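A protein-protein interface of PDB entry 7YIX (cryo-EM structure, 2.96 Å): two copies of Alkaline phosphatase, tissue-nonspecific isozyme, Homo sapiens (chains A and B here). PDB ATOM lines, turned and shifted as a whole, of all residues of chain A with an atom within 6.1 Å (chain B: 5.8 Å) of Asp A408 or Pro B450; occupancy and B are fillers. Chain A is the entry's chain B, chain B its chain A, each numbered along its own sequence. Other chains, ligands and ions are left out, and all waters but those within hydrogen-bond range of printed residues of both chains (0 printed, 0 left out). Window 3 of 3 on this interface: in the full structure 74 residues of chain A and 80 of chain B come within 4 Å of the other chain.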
ATOM      1  N   SER A 405      19.072 -14.694 -26.295  1.00  0.00           N
ATOM      2  CA  SER A 405      20.126 -15.493 -26.900  1.00  0.00           C
ATOM      3  C   SER A 405      20.078 -15.376 -28.417  1.00  0.00           C
ATOM      4  O   SER A 405      19.004 -15.253 -29.014  1.00  0.00           O
ATOM      5  CB  SER A 405      19.995 -16.952 -26.476  1.00  0.00           C
ATOM      6  OG  SER A 405      20.900 -17.770 -27.195  1.00  0.00           O
ATOM      7  N   ASP A 406      21.256 -15.413 -29.043  1.00  0.00           N
ATOM      8  CA  ASP A 406      21.345 -15.247 -30.489  1.00  0.00           C
ATOM      9  C   ASP A 406      20.896 -16.486 -31.251  1.00  0.00           C
ATOM     10  O   ASP A 406      20.486 -16.367 -32.410  1.00  0.00           O
ATOM     11  CB  ASP A 406      22.777 -14.892 -30.888  1.00  0.00           C
ATOM     12  CG  ASP A 406      23.336 -13.733 -30.089  1.00  0.00           C
ATOM     13  OD1 ASP A 406      24.553 -13.472 -30.185  1.00  0.00           O
ATOM     14  OD2 ASP A 406      22.559 -13.085 -29.358  1.00  0.00           O
ATOM     15  N   THR A 407      20.959 -17.666 -30.634  1.00  0.00           N
ATOM     16  CA  THR A 407      20.729 -18.926 -31.336  1.00  0.00           C
ATOM     17  C   THR A 407      19.313 -19.462 -31.146  1.00  0.00           C
ATOM     18  O   THR A 407      18.595 -19.678 -32.126  1.00  0.00           O
ATOM     19  CB  THR A 407      21.753 -19.970 -30.879  1.00  0.00           C
ATOM     20  OG1 THR A 407      23.051 -19.367 -30.808  1.00  0.00           O
ATOM     21  CG2 THR A 407      21.794 -21.133 -31.854  1.00  0.00           C
ATOM     22  N   ASP A 408      18.898 -19.689 -29.900  1.00  0.00           N
ATOM     23  CA  ASP A 408      17.594 -20.276 -29.618  1.00  0.00           C
ATOM     24  C   ASP A 408      16.554 -19.256 -29.177  1.00  0.00           C
ATOM     25  O   ASP A 408      15.393 -19.627 -28.984  1.00  0.00           O
ATOM     26  CB  ASP A 408      17.729 -21.377 -28.561  1.00  0.00           C
ATOM     27  CG  ASP A 408      18.587 -20.958 -27.393  1.00  0.00           C
ATOM     28  OD1 ASP A 408      19.104 -19.824 -27.416  1.00  0.00           O
ATOM     29  OD2 ASP A 408      18.750 -21.764 -26.453  1.00  0.00           O
ATOM     30  N   LYS A 409      16.940 -17.989 -29.015  1.00  0.00           N
ATOM     31  CA  LYS A 409      16.012 -16.891 -28.739  1.00  0.00           C
ATOM     32  C   LYS A 409      15.253 -17.112 -27.427  1.00  0.00           C
ATOM     33  O   LYS A 409      14.024 -17.186 -27.391  1.00  0.00           O
ATOM     34  CB  LYS A 409      15.044 -16.695 -29.910  1.00  0.00           C
ATOM     35  CG  LYS A 409      15.722 -16.320 -31.215  1.00  0.00           C
ATOM     36  CD  LYS A 409      15.061 -17.010 -32.393  1.00  0.00           C
ATOM     37  CE  LYS A 409      15.805 -16.725 -33.686  1.00  0.00           C
ATOM     38  NZ  LYS A 409      17.260 -17.012 -33.561  1.00  0.00           N
ATOM     39  N   LYS A 410      16.014 -17.211 -26.344  1.00  0.00           N
ATOM     40  CA  LYS A 410      15.463 -17.348 -25.006  1.00  0.00           C
ATOM     41  C   LYS A 410      16.269 -16.494 -24.042  1.00  0.00           C
ATOM     42  O   LYS A 410      17.475 -16.307 -24.235  1.00  0.00           O
ATOM     43  CB  LYS A 410      15.474 -18.812 -24.537  1.00  0.00           C
ATOM     44  CG  LYS A 410      14.400 -19.665 -25.177  1.00  0.00           C
ATOM     45  CD  LYS A 410      14.610 -21.134 -24.889  1.00  0.00           C
ATOM     46  CE  LYS A 410      13.604 -21.972 -25.649  1.00  0.00           C
ATOM     47  NZ  LYS A 410      13.867 -23.422 -25.504  1.00  0.00           N
ATOM     48  N   ARG A 430      16.979 -26.017 -23.589  1.00  0.00           N
ATOM     49  CA  ARG A 430      17.247 -25.516 -22.251  1.00  0.00           C
ATOM     50  C   ARG A 430      16.046 -24.732 -21.729  1.00  0.00           C
ATOM     51  O   ARG A 430      15.149 -24.341 -22.480  1.00  0.00           O
ATOM     52  CB  ARG A 430      18.505 -24.650 -22.235  1.00  0.00           C
ATOM     53  CG  ARG A 430      18.362 -23.316 -22.919  1.00  0.00           C
ATOM     54  CD  ARG A 430      19.560 -22.434 -22.631  1.00  0.00           C
ATOM     55  NE  ARG A 430      19.486 -21.176 -23.362  1.00  0.00           N
ATOM     56  CZ  ARG A 430      18.877 -20.085 -22.920  1.00  0.00           C
ATOM     57  NH1 ARG A 430      18.291 -20.052 -21.734  1.00  0.00           N
ATOM     58  NH2 ARG A 430      18.861 -18.997 -23.683  1.00  0.00           N
ATOM     59  N   GLY B 420      28.793 -18.907 -24.701  1.00  0.00           N
ATOM     60  CA  GLY B 420      29.532 -18.808 -25.936  1.00  0.00           C
ATOM     61  C   GLY B 420      29.027 -19.740 -27.015  1.00  0.00           C
ATOM     62  O   GLY B 420      27.930 -20.298 -26.925  1.00  0.00           O
ATOM     63  N   PRO B 421      29.825 -19.920 -28.070  1.00  0.00           N
ATOM     64  CA  PRO B 421      29.450 -20.841 -29.147  1.00  0.00           C
ATOM     65  C   PRO B 421      29.837 -22.289 -28.895  1.00  0.00           C
ATOM     66  O   PRO B 421      29.619 -23.129 -29.774  1.00  0.00           O
ATOM     67  CB  PRO B 421      30.210 -20.274 -30.349  1.00  0.00           C
ATOM     68  CG  PRO B 421      31.426 -19.671 -29.756  1.00  0.00           C
ATOM     69  CD  PRO B 421      31.069 -19.192 -28.374  1.00  0.00           C
ATOM     70  N   TYR B 423      28.432 -24.265 -26.718  1.00  0.00           N
ATOM     71  CA  TYR B 423      27.267 -25.019 -26.273  1.00  0.00           C
ATOM     72  C   TYR B 423      26.846 -26.030 -27.329  1.00  0.00           C
ATOM     73  O   TYR B 423      26.338 -25.651 -28.389  1.00  0.00           O
ATOM     74  CB  TYR B 423      26.115 -24.063 -25.950  1.00  0.00           C
ATOM     75  CG  TYR B 423      24.813 -24.726 -25.546  1.00  0.00           C
ATOM     76  CD1 TYR B 423      23.866 -25.079 -26.496  1.00  0.00           C
ATOM     77  CD2 TYR B 423      24.521 -24.974 -24.213  1.00  0.00           C
ATOM     78  CE1 TYR B 423      22.678 -25.674 -26.134  1.00  0.00           C
ATOM     79  CE2 TYR B 423      23.334 -25.566 -23.843  1.00  0.00           C
ATOM     80  CZ  TYR B 423      22.417 -25.913 -24.808  1.00  0.00           C
ATOM     81  OH  TYR B 423      21.231 -26.506 -24.449  1.00  0.00           O
ATOM     82  N   SER B 447      29.600 -24.749 -22.852  1.00  0.00           N
ATOM     83  CA  SER B 447      29.107 -23.570 -22.157  1.00  0.00           C
ATOM     84  C   SER B 447      27.670 -23.802 -21.711  1.00  0.00           C
ATOM     85  O   SER B 447      27.032 -24.790 -22.083  1.00  0.00           O
ATOM     86  CB  SER B 447      29.191 -22.327 -23.045  1.00  0.00           C
ATOM     87  OG  SER B 447      28.319 -22.446 -24.153  1.00  0.00           O
ATOM     88  N   ALA B 448      27.162 -22.865 -20.910  1.00  0.00           N
ATOM     89  CA  ALA B 448      25.844 -22.984 -20.293  1.00  0.00           C
ATOM     90  C   ALA B 448      24.719 -22.504 -21.204  1.00  0.00           C
ATOM     91  O   ALA B 448      23.732 -23.218 -21.399  1.00  0.00           O
ATOM     92  CB  ALA B 448      25.815 -22.208 -18.975  1.00  0.00           C
ATOM     93  N   VAL B 449      24.846 -21.302 -21.758  1.00  0.00           N
ATOM     94  CA  VAL B 449      23.819 -20.728 -22.627  1.00  0.00           C
ATOM     95  C   VAL B 449      24.412 -20.491 -24.013  1.00  0.00           C
ATOM     96  O   VAL B 449      25.547 -20.007 -24.128  1.00  0.00           O
ATOM     97  CB  VAL B 449      23.231 -19.445 -22.013  1.00  0.00           C
ATOM     98  CG1 VAL B 449      24.271 -18.360 -21.910  1.00  0.00           C
ATOM     99  CG2 VAL B 449      22.060 -18.949 -22.827  1.00  0.00           C
ATOM    100  N   PRO B 450      23.709 -20.853 -25.089  1.00  0.00           N
ATOM    101  CA  PRO B 450      24.283 -20.702 -26.432  1.00  0.00           C
ATOM    102  C   PRO B 450      24.279 -19.248 -26.884  1.00  0.00           C
ATOM    103  O   PRO B 450      23.264 -18.556 -26.798  1.00  0.00           O
ATOM    104  CB  PRO B 450      23.363 -21.558 -27.308  1.00  0.00           C
ATOM    105  CG  PRO B 450      22.077 -21.569 -26.586  1.00  0.00           C
ATOM    106  CD  PRO B 450      22.425 -21.572 -25.126  1.00  0.00           C
ATOM    107  N   LEU B 451      25.429 -18.794 -27.375  1.00  0.00           N
ATOM    108  CA  LEU B 451      25.575 -17.468 -27.948  1.00  0.00           C
ATOM    109  C   LEU B 451      26.498 -17.572 -29.151  1.00  0.00           C
ATOM    110  O   LEU B 451      27.011 -18.645 -29.474  1.00  0.00           O
ATOM    111  CB  LEU B 451      26.130 -16.462 -26.931  1.00  0.00           C
ATOM    112  CG  LEU B 451      25.205 -15.996 -25.809  1.00  0.00           C
ATOM    113  CD1 LEU B 451      25.924 -15.016 -24.905  1.00  0.00           C
ATOM    114  CD2 LEU B 451      23.957 -15.373 -26.383  1.00  0.00           C
ATOM    115  N   ARG B 452      26.698 -16.445 -29.827  1.00  0.00           N
ATOM    116  CA  ARG B 452      27.658 -16.382 -30.917  1.00  0.00           C
ATOM    117  C   ARG B 452      28.996 -15.798 -30.489  1.00  0.00           C
ATOM    118  O   ARG B 452      29.969 -15.903 -31.242  1.00  0.00           O
ATOM    119  CB  ARG B 452      27.090 -15.561 -32.077  1.00  0.00           C
ATOM    120  CG  ARG B 452      25.904 -16.213 -32.758  1.00  0.00           C
ATOM    121  CD  ARG B 452      25.398 -15.379 -33.923  1.00  0.00           C
ATOM    122  NE  ARG B 452      24.199 -15.955 -34.522  1.00  0.00           N
ATOM    123  CZ  ARG B 452      24.199 -16.848 -35.501  1.00  0.00           C
ATOM    124  NH1 ARG B 452      25.326 -17.298 -36.027  1.00  0.00           N
ATOM    125  NH2 ARG B 452      23.037 -17.300 -35.967  1.00  0.00           N
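No position is printed for both chains.
Of the 9 printed residues of chain B, 5 touch a printed residue of chain A. Hydrophobic or aromatic side chains of chain B within 4 Å of the printed part of chain A: Tyr B423, Val B449, Pro B450 and Leu B451. Among the printed residues, 8 pairs touch across the chains. Among the printed residues, no Asp or Glu carboxylate lies within 4 Å of a Lys or Arg side-chain nitrogen of the other chain.
Of the printed residues of chain B, Asp A406 touches Leu B451 (3.8 Å) and Arg B452 (3.7 Å). Asp A408 touches one residue of chain B. Printed residues of chain B within 4 Å of Arg A430: Tyr B423 (3.97 Å), Val B449 (3.3 Å) and Pro B450 (3.5 Å). Ala B448 touches none of the printed residues of chain A. Of the printed residues of chain A, Val B449 touches Arg A430 (3.3 Å). Pro B450 touches three residues of chain A. Of the printed residues of chain A, Leu B451 touches Ser A405 (3.9 Å) and Asp A406 (3.8 Å). The nearest printed residue of chain B that does not touch Asp A408 is Val B449 (5.5 Å). The nearest printed residue of chain A that does not touch Val B449 is Ser A405 (4.6 Å).
O of Gly B420 is in hydrogen-bond range of N of Leu B451 (3.0 Å). N of Gly B420 sits at hydrogen-bond distance from O of Val B449, 3.5 Å away. The backbone NH (N) of Thr A407 lies close to the side-chain hydroxyl (OG) of Ser A405 (3.4 Å). The side-chain amino group (NZ) of Lys A409 lies within hydrogen-bond range of the backbone carbonyl oxygen (O) of Asp A406 (3.5 Å). The backbone NH of Ser A405 sits at hydrogen-bond distance from the backbone carbonyl oxygen of Lys A410. OD2 of Asp A408 lies within salt-bridge range of NE of Arg A430, at 3.2 Å.
Ser A405 touches Leu B451. Leu B451 touches Asp A406. Asp A406 touches Arg B452 (OD1 to N, 3.7 Å). Asp A408 touches Pro B450 (OD2 to CG, 3.3 Å). Arg A430 touches Tyr B423. CG2 of Val B449 touches NH2 of Arg A430, 3.3 Å away. Arg A430 touches Pro B450.
The backbone carbonyl oxygen (O) of Pro B450 is in hydrogen-bond range of the side-chain hydroxyl (OG) of Ser A405 (2.5 Å).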
